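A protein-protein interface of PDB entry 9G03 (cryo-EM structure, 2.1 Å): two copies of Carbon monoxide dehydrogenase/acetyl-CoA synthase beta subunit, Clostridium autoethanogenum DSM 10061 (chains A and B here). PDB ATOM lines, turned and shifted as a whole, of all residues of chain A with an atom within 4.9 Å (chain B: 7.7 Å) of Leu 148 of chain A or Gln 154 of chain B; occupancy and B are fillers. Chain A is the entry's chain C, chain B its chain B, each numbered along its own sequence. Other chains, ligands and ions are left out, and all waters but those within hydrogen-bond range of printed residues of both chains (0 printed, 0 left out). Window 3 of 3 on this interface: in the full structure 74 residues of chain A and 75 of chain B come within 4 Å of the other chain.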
ATOM      1  N   ARG A  97       1.263  -7.348 -23.482  1.00  0.00           N
ATOM      2  CA  ARG A  97       0.358  -8.366 -24.006  1.00  0.00           C
ATOM      3  C   ARG A  97      -0.887  -8.498 -23.137  1.00  0.00           C
ATOM      4  O   ARG A  97      -2.006  -8.597 -23.653  1.00  0.00           O
ATOM      5  CB  ARG A  97       1.079  -9.711 -24.086  1.00  0.00           C
ATOM      6  CG  ARG A  97       0.328 -10.807 -24.831  1.00  0.00           C
ATOM      7  CD  ARG A  97       0.708 -12.202 -24.325  1.00  0.00           C
ATOM      8  NE  ARG A  97       2.136 -12.318 -24.048  1.00  0.00           N
ATOM      9  CZ  ARG A  97       3.073 -12.502 -24.966  1.00  0.00           C
ATOM     10  NH1 ARG A  97       2.773 -12.633 -26.246  1.00  0.00           N
ATOM     11  NH2 ARG A  97       4.347 -12.532 -24.594  1.00  0.00           N
ATOM     12  N   ALA A 100      -3.058  -5.568 -23.964  1.00  0.00           N
ATOM     13  CA  ALA A 100      -3.725  -5.715 -25.257  1.00  0.00           C
ATOM     14  C   ALA A 100      -4.889  -6.697 -25.172  1.00  0.00           C
ATOM     15  O   ALA A 100      -5.957  -6.454 -25.744  1.00  0.00           O
ATOM     16  CB  ALA A 100      -2.723  -6.156 -26.321  1.00  0.00           C
ATOM     17  N   LEU A 101      -4.709  -7.799 -24.443  1.00  0.00           N
ATOM     18  CA  LEU A 101      -5.807  -8.743 -24.255  1.00  0.00           C
ATOM     19  C   LEU A 101      -6.960  -8.090 -23.499  1.00  0.00           C
ATOM     20  O   LEU A 101      -8.125  -8.271 -23.861  1.00  0.00           O
ATOM     21  CB  LEU A 101      -5.309 -10.000 -23.527  1.00  0.00           C
ATOM     22  CG  LEU A 101      -4.337 -10.895 -24.317  1.00  0.00           C
ATOM     23  CD1 LEU A 101      -3.771 -12.008 -23.460  1.00  0.00           C
ATOM     24  CD2 LEU A 101      -5.009 -11.486 -25.557  1.00  0.00           C
ATOM     25  N   TYR A 104      -8.844  -6.072 -25.898  1.00  0.00           N
ATOM     26  CA  TYR A 104      -9.675  -6.909 -26.751  1.00  0.00           C
ATOM     27  C   TYR A 104     -10.972  -7.321 -26.060  1.00  0.00           C
ATOM     28  O   TYR A 104     -11.983  -7.539 -26.732  1.00  0.00           O
ATOM     29  CB  TYR A 104      -8.884  -8.144 -27.166  1.00  0.00           C
ATOM     30  CG  TYR A 104      -9.596  -9.023 -28.145  1.00  0.00           C
ATOM     31  CD1 TYR A 104      -9.789  -8.617 -29.455  1.00  0.00           C
ATOM     32  CD2 TYR A 104     -10.067 -10.267 -27.766  1.00  0.00           C
ATOM     33  CE1 TYR A 104     -10.435  -9.419 -30.353  1.00  0.00           C
ATOM     34  CE2 TYR A 104     -10.712 -11.078 -28.659  1.00  0.00           C
ATOM     35  CZ  TYR A 104     -10.895 -10.651 -29.954  1.00  0.00           C
ATOM     36  OH  TYR A 104     -11.543 -11.463 -30.848  1.00  0.00           O
ATOM     37  N   ALA A 144      -6.903  -3.757 -30.728  1.00  0.00           N
ATOM     38  CA  ALA A 144      -6.289  -4.798 -29.912  1.00  0.00           C
ATOM     39  C   ALA A 144      -5.774  -5.947 -30.771  1.00  0.00           C
ATOM     40  O   ALA A 144      -4.692  -6.477 -30.511  1.00  0.00           O
ATOM     41  CB  ALA A 144      -7.291  -5.305 -28.874  1.00  0.00           C
ATOM     42  N   LYS A 145      -6.515  -6.318 -31.816  1.00  0.00           N
ATOM     43  CA  LYS A 145      -6.049  -7.365 -32.724  1.00  0.00           C
ATOM     44  C   LYS A 145      -4.744  -6.969 -33.408  1.00  0.00           C
ATOM     45  O   LYS A 145      -3.807  -7.770 -33.480  1.00  0.00           O
ATOM     46  CB  LYS A 145      -7.118  -7.676 -33.777  1.00  0.00           C
ATOM     47  CG  LYS A 145      -8.416  -8.218 -33.228  1.00  0.00           C
ATOM     48  CD  LYS A 145      -9.580  -7.920 -34.177  1.00  0.00           C
ATOM     49  CE  LYS A 145     -10.930  -8.015 -33.487  1.00  0.00           C
ATOM     50  NZ  LYS A 145     -12.009  -7.396 -34.294  1.00  0.00           N
ATOM     51  N   GLU A 146      -4.655  -5.731 -33.897  1.00  0.00           N
ATOM     52  CA  GLU A 146      -3.414  -5.275 -34.530  1.00  0.00           C
ATOM     53  C   GLU A 146      -2.253  -5.270 -33.538  1.00  0.00           C
ATOM     54  O   GLU A 146      -1.138  -5.717 -33.857  1.00  0.00           O
ATOM     55  CB  GLU A 146      -3.600  -3.881 -35.125  1.00  0.00           C
ATOM     56  CG  GLU A 146      -4.639  -3.806 -36.210  1.00  0.00           C
ATOM     57  CD  GLU A 146      -4.323  -4.704 -37.387  1.00  0.00           C
ATOM     58  OE1 GLU A 146      -3.149  -4.747 -37.812  1.00  0.00           O
ATOM     59  OE2 GLU A 146      -5.250  -5.376 -37.883  1.00  0.00           O
ATOM     60  N   GLY A 147      -2.504  -4.793 -32.319  1.00  0.00           N
ATOM     61  CA  GLY A 147      -1.467  -4.792 -31.301  1.00  0.00           C
ATOM     62  C   GLY A 147      -0.982  -6.190 -30.966  1.00  0.00           C
ATOM     63  O   GLY A 147       0.220  -6.436 -30.875  1.00  0.00           O
ATOM     64  N   LEU A 148      -1.911  -7.135 -30.833  1.00  0.00           N
ATOM     65  CA  LEU A 148      -1.546  -8.523 -30.571  1.00  0.00           C
ATOM     66  C   LEU A 148      -0.748  -9.112 -31.726  1.00  0.00           C
ATOM     67  O   LEU A 148       0.236  -9.823 -31.506  1.00  0.00           O
ATOM     68  CB  LEU A 148      -2.796  -9.364 -30.308  1.00  0.00           C
ATOM     69  CG  LEU A 148      -3.501  -9.129 -28.968  1.00  0.00           C
ATOM     70  CD1 LEU A 148      -4.858  -9.796 -28.955  1.00  0.00           C
ATOM     71  CD2 LEU A 148      -2.658  -9.613 -27.806  1.00  0.00           C
ATOM     72  N   SER A 149      -1.113  -8.775 -32.958  1.00  0.00           N
ATOM     73  CA  SER A 149      -0.345  -9.260 -34.098  1.00  0.00           C
ATOM     74  C   SER A 149       1.087  -8.739 -34.042  1.00  0.00           C
ATOM     75  O   SER A 149       2.012  -9.430 -34.475  1.00  0.00           O
ATOM     76  CB  SER A 149      -1.028  -8.877 -35.410  1.00  0.00           C
ATOM     77  OG  SER A 149      -0.822  -7.525 -35.747  1.00  0.00           O
ATOM     78  N   ASN A 150       1.292  -7.546 -33.488  1.00  0.00           N
ATOM     79  CA  ASN A 150       2.661  -7.056 -33.320  1.00  0.00           C
ATOM     80  C   ASN A 150       3.509  -8.023 -32.491  1.00  0.00           C
ATOM     81  O   ASN A 150       4.730  -8.060 -32.651  1.00  0.00           O
ATOM     82  CB  ASN A 150       2.671  -5.673 -32.664  1.00  0.00           C
ATOM     83  CG  ASN A 150       2.924  -4.565 -33.649  1.00  0.00           C
ATOM     84  OD1 ASN A 150       3.028  -4.800 -34.848  1.00  0.00           O
ATOM     85  ND2 ASN A 150       3.017  -3.341 -33.147  1.00  0.00           N
ATOM     86  N   TYR A 151       2.895  -8.798 -31.595  1.00  0.00           N
ATOM     87  CA  TYR A 151       3.672  -9.676 -30.723  1.00  0.00           C
ATOM     88  C   TYR A 151       4.141 -10.943 -31.434  1.00  0.00           C
ATOM     89  O   TYR A 151       5.227 -11.438 -31.122  1.00  0.00           O
ATOM     90  CB  TYR A 151       2.867 -10.042 -29.476  1.00  0.00           C
ATOM     91  CG  TYR A 151       2.805  -8.908 -28.487  1.00  0.00           C
ATOM     92  CD1 TYR A 151       3.785  -8.756 -27.518  1.00  0.00           C
ATOM     93  CD2 TYR A 151       1.789  -7.971 -28.541  1.00  0.00           C
ATOM     94  CE1 TYR A 151       3.748  -7.711 -26.628  1.00  0.00           C
ATOM     95  CE2 TYR A 151       1.739  -6.930 -27.648  1.00  0.00           C
ATOM     96  CZ  TYR A 151       2.728  -6.805 -26.694  1.00  0.00           C
ATOM     97  OH  TYR A 151       2.689  -5.768 -25.804  1.00  0.00           O
ATOM     98  N   GLY A 152       3.357 -11.498 -32.355  1.00  0.00           N
ATOM     99  CA  GLY A 152       3.673 -12.821 -32.856  1.00  0.00           C
ATOM    100  C   GLY A 152       3.530 -13.040 -34.351  1.00  0.00           C
ATOM    101  O   GLY A 152       3.487 -14.191 -34.790  1.00  0.00           O
ATOM    102  N   ASP A 183       7.950 -11.424 -29.457  1.00  0.00           N
ATOM    103  CA  ASP A 183       8.294 -12.766 -28.993  1.00  0.00           C
ATOM    104  C   ASP A 183       9.283 -13.445 -29.935  1.00  0.00           C
ATOM    105  O   ASP A 183      10.173 -14.167 -29.480  1.00  0.00           O
ATOM    106  CB  ASP A 183       7.033 -13.615 -28.824  1.00  0.00           C
ATOM    107  CG  ASP A 183       6.036 -13.020 -27.838  1.00  0.00           C
ATOM    108  OD1 ASP A 183       6.445 -12.325 -26.882  1.00  0.00           O
ATOM    109  OD2 ASP A 183       4.827 -13.261 -28.015  1.00  0.00           O
ATOM    110  N   SER B 149       1.401 -19.823 -37.731  1.00  0.00           N
ATOM    111  CA  SER B 149       0.489 -19.313 -36.714  1.00  0.00           C
ATOM    112  C   SER B 149       0.683 -20.050 -35.391  1.00  0.00           C
ATOM    113  O   SER B 149       0.535 -19.449 -34.325  1.00  0.00           O
ATOM    114  CB  SER B 149      -0.960 -19.415 -37.189  1.00  0.00           C
ATOM    115  OG  SER B 149      -1.456 -20.734 -37.112  1.00  0.00           O
ATOM    116  N   TYR B 151       3.364 -20.609 -34.038  1.00  0.00           N
ATOM    117  CA  TYR B 151       4.467 -19.983 -33.316  1.00  0.00           C
ATOM    118  C   TYR B 151       4.061 -18.714 -32.568  1.00  0.00           C
ATOM    119  O   TYR B 151       4.611 -18.447 -31.495  1.00  0.00           O
ATOM    120  CB  TYR B 151       5.606 -19.658 -34.281  1.00  0.00           C
ATOM    121  CG  TYR B 151       6.387 -20.882 -34.678  1.00  0.00           C
ATOM    122  CD1 TYR B 151       7.480 -21.302 -33.935  1.00  0.00           C
ATOM    123  CD2 TYR B 151       6.016 -21.640 -35.778  1.00  0.00           C
ATOM    124  CE1 TYR B 151       8.188 -22.436 -34.279  1.00  0.00           C
ATOM    125  CE2 TYR B 151       6.725 -22.772 -36.134  1.00  0.00           C
ATOM    126  CZ  TYR B 151       7.808 -23.162 -35.379  1.00  0.00           C
ATOM    127  OH  TYR B 151       8.510 -24.284 -35.729  1.00  0.00           O
ATOM    128  N   GLY B 152       3.133 -17.921 -33.096  1.00  0.00           N
ATOM    129  CA  GLY B 152       2.902 -16.603 -32.530  1.00  0.00           C
ATOM    130  C   GLY B 152       1.457 -16.166 -32.384  1.00  0.00           C
ATOM    131  O   GLY B 152       1.196 -14.980 -32.171  1.00  0.00           O
ATOM    132  N   LYS B 153       0.509 -17.095 -32.455  1.00  0.00           N
ATOM    133  CA  LYS B 153      -0.890 -16.740 -32.264  1.00  0.00           C
ATOM    134  C   LYS B 153      -1.139 -16.298 -30.826  1.00  0.00           C
ATOM    135  O   LYS B 153      -0.643 -16.906 -29.875  1.00  0.00           O
ATOM    136  CB  LYS B 153      -1.808 -17.911 -32.623  1.00  0.00           C
ATOM    137  CG  LYS B 153      -1.610 -19.176 -31.803  1.00  0.00           C
ATOM    138  CD  LYS B 153      -2.926 -19.899 -31.562  1.00  0.00           C
ATOM    139  CE  LYS B 153      -3.627 -20.270 -32.852  1.00  0.00           C
ATOM    140  NZ  LYS B 153      -2.799 -21.165 -33.695  1.00  0.00           N
ATOM    141  N   GLN B 154      -1.908 -15.224 -30.671  1.00  0.00           N
ATOM    142  CA  GLN B 154      -2.235 -14.698 -29.355  1.00  0.00           C
ATOM    143  C   GLN B 154      -3.658 -15.011 -28.922  1.00  0.00           C
ATOM    144  O   GLN B 154      -3.963 -14.910 -27.732  1.00  0.00           O
ATOM    145  CB  GLN B 154      -2.014 -13.181 -29.338  1.00  0.00           C
ATOM    146  CG  GLN B 154      -0.614 -12.774 -29.756  1.00  0.00           C
ATOM    147  CD  GLN B 154       0.463 -13.333 -28.844  1.00  0.00           C
ATOM    148  OE1 GLN B 154       0.386 -13.207 -27.624  1.00  0.00           O
ATOM    149  NE2 GLN B 154       1.481 -13.939 -29.435  1.00  0.00           N
ATOM    150  N   LEU B 155      -4.528 -15.382 -29.855  1.00  0.00           N
ATOM    151  CA  LEU B 155      -5.897 -15.784 -29.571  1.00  0.00           C
ATOM    152  C   LEU B 155      -6.126 -17.196 -30.091  1.00  0.00           C
ATOM    153  O   LEU B 155      -5.625 -17.557 -31.158  1.00  0.00           O
ATOM    154  CB  LEU B 155      -6.904 -14.820 -30.209  1.00  0.00           C
ATOM    155  CG  LEU B 155      -6.818 -13.362 -29.759  1.00  0.00           C
ATOM    156  CD1 LEU B 155      -7.789 -12.499 -30.545  1.00  0.00           C
ATOM    157  CD2 LEU B 155      -7.080 -13.235 -28.268  1.00  0.00           C
ATOM    158  N   GLY B 156      -6.871 -17.991 -29.335  1.00  0.00           N
ATOM    159  CA  GLY B 156      -7.207 -19.339 -29.746  1.00  0.00           C
ATOM    160  C   GLY B 156      -6.210 -20.379 -29.284  1.00  0.00           C
ATOM    161  O   GLY B 156      -5.216 -20.101 -28.609  1.00  0.00           O
ATOM    162  N   GLU B 157      -6.489 -21.616 -29.679  1.00  0.00           N
ATOM    163  CA  GLU B 157      -5.678 -22.763 -29.309  1.00  0.00           C
ATOM    164  C   GLU B 157      -4.754 -23.169 -30.451  1.00  0.00           C
ATOM    165  O   GLU B 157      -5.079 -23.005 -31.627  1.00  0.00           O
ATOM    166  CB  GLU B 157      -6.570 -23.945 -28.916  1.00  0.00           C
ATOM    167  CG  GLU B 157      -5.811 -25.133 -28.340  1.00  0.00           C
ATOM    168  CD  GLU B 157      -6.547 -26.444 -28.505  1.00  0.00           C
ATOM    169  OE1 GLU B 157      -7.708 -26.542 -28.053  1.00  0.00           O
ATOM    170  OE2 GLU B 157      -5.960 -27.376 -29.094  1.00  0.00           O
ATOM    171  N   ARG B 180       0.679 -23.128 -25.304  1.00  0.00           N
ATOM    172  CA  ARG B 180       0.288 -21.994 -26.124  1.00  0.00           C
ATOM    173  C   ARG B 180       1.312 -21.848 -27.252  1.00  0.00           C
ATOM    174  O   ARG B 180       2.134 -22.737 -27.481  1.00  0.00           O
ATOM    175  CB  ARG B 180       0.159 -20.740 -25.252  1.00  0.00           C
ATOM    176  CG  ARG B 180      -0.902 -20.867 -24.163  1.00  0.00           C
ATOM    177  CD  ARG B 180      -0.825 -19.757 -23.123  1.00  0.00           C
ATOM    178  NE  ARG B 180       0.443 -19.739 -22.403  1.00  0.00           N
ATOM    179  CZ  ARG B 180       0.733 -18.900 -21.418  1.00  0.00           C
ATOM    180  NH1 ARG B 180      -0.151 -18.019 -20.977  1.00  0.00           N
ATOM    181  NH2 ARG B 180       1.944 -18.935 -20.871  1.00  0.00           N
ATOM    182  N   ALA B 181       1.231 -20.742 -27.988  1.00  0.00           N
ATOM    183  CA  ALA B 181       2.188 -20.474 -29.056  1.00  0.00           C
ATOM    184  C   ALA B 181       3.623 -20.506 -28.524  1.00  0.00           C
ATOM    185  O   ALA B 181       3.896 -20.077 -27.399  1.00  0.00           O
ATOM    186  CB  ALA B 181       1.887 -19.124 -29.701  1.00  0.00           C
ATOM    187  N   ASP B 183       6.684 -19.098 -29.145  1.00  0.00           N
ATOM    188  CA  ASP B 183       7.396 -17.893 -28.724  1.00  0.00           C
ATOM    189  C   ASP B 183       6.741 -17.261 -27.502  1.00  0.00           C
ATOM    190  O   ASP B 183       7.437 -16.739 -26.627  1.00  0.00           O
ATOM    191  CB  ASP B 183       7.476 -16.893 -29.879  1.00  0.00           C
ATOM    192  CG  ASP B 183       8.228 -17.438 -31.080  1.00  0.00           C
ATOM    193  OD1 ASP B 183       9.122 -18.292 -30.903  1.00  0.00           O
ATOM    194  OD2 ASP B 183       7.931 -17.001 -32.206  1.00  0.00           O
ATOM    195  N   ARG B 184       5.414 -17.346 -27.405  1.00  0.00           N
ATOM    196  CA  ARG B 184       4.711 -16.852 -26.229  1.00  0.00           C
ATOM    197  C   ARG B 184       5.153 -17.590 -24.967  1.00  0.00           C
ATOM    198  O   ARG B 184       5.355 -16.970 -23.923  1.00  0.00           O
ATOM    199  CB  ARG B 184       3.200 -16.985 -26.435  1.00  0.00           C
ATOM    200  CG  ARG B 184       2.351 -16.154 -25.490  1.00  0.00           C
ATOM    201  CD  ARG B 184       1.889 -16.951 -24.290  1.00  0.00           C
ATOM    202  NE  ARG B 184       1.210 -16.108 -23.317  1.00  0.00           N
ATOM    203  CZ  ARG B 184       1.833 -15.318 -22.454  1.00  0.00           C
ATOM    204  NH1 ARG B 184       3.154 -15.231 -22.421  1.00  0.00           N
ATOM    205  NH2 ARG B 184       1.113 -14.585 -21.613  1.00  0.00           N
ATOM    206  N   GLU B 185       5.329 -18.909 -25.049  1.00  0.00           N
ATOM    207  CA  GLU B 185       5.741 -19.673 -23.872  1.00  0.00           C
ATOM    208  C   GLU B 185       7.188 -19.377 -23.492  1.00  0.00           C
ATOM    209  O   GLU B 185       7.514 -19.289 -22.301  1.00  0.00           O
ATOM    210  CB  GLU B 185       5.541 -21.167 -24.111  1.00  0.00           C
ATOM    211  CG  GLU B 185       4.086 -21.579 -24.229  1.00  0.00           C
ATOM    212  CD  GLU B 185       3.316 -21.467 -22.933  1.00  0.00           C
ATOM    213  OE1 GLU B 185       3.921 -21.163 -21.888  1.00  0.00           O
ATOM    214  OE2 GLU B 185       2.092 -21.688 -22.960  1.00  0.00           O
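The side-chain amide oxygen (OE1) of Gln 154 of chain B is in hydrogen-bond range of the guanidinium group (NH1) of Arg 97 of chain A, 2.8 Å away.
NH2 of Arg 184 of chain B lies close to NE of Arg 97 of chain A (3.5 Å).
The backbone carbonyl oxygen (O) of Tyr 151 of chain B lies within hydrogen-bond range of the backbone NH (N) of Asp 183 of chain B, 3.2 Å away.
The backbone carbonyl oxygen (O) of Gly 152 of chain B is in hydrogen-bond range of the side-chain amide nitrogen (NE2) of Gln 154 of chain B.
The backbone NH of Arg 97 of chain A lies within hydrogen-bond range of the side-chain hydroxyl of Tyr 151 of chain A (3.1 Å).
NH1 of Arg 97 of chain A lies within salt-bridge range of OD2 of Asp 183 of chain A, at 2.8 Å.
N of Asp 183 of chain A sits at hydrogen-bond distance from O of Tyr 151 of chain A (3.2 Å).
Among the printed residues, pairs that only touch across the chains: Leu 101 of chain A with Leu 155 of chain B, Tyr 104 of chain A with Leu 155 of chain B, Leu 148 of chain A with Gln 154 of chain B, Gly 152 of chain A with Gly 152 of chain B, Asp 183 of chain A with Gln 154 of chain B and Asp 183 of chain A with Asp 183 of chain B.
No residue of chain B comes within 4 Å of Gly 147 of chain A.
Printed residues of chain B within 4 Å of Asp 183 of chain A: Gln 154 and Asp 183.
Of the printed residues of chain A, Gly 152 of chain B touches Gly 152.
Of the printed residues of chain B, Tyr 104 of chain A touches Leu 155 (3.7 Å).
Printed residues of chain B within 4 Å of Gly 152 of chain A: Gly 152.
Gly 156 of chain B touches none of the printed residues of chain A.
Asn 150 of chain A touches none of the printed residues of chain B.
The nearest residue of chain B that does not touch Leu 148 of chain A is Leu 155 of chain B (4.1 Å).
Of the 13 printed residues of chain B, 5 touch a printed residue of chain A.
Hydrophobic or aromatic side chains of chain B within 4 Å of the printed part of chain A: Leu 155.
Of the 14 printed residues of chain A, 6 touch a printed residue of chain B.
Among the printed residues, 8 pairs touch across the chains.
Gly 152 of chain A touches its own counterpart, Gly 152 of chain B.
Asp 183 of chain B touches its own counterpart, Asp 183 of chain A.
Of the 8 pairs that touch across the chains among the printed residues, 2 have their exchanged pair printed and touching as well.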
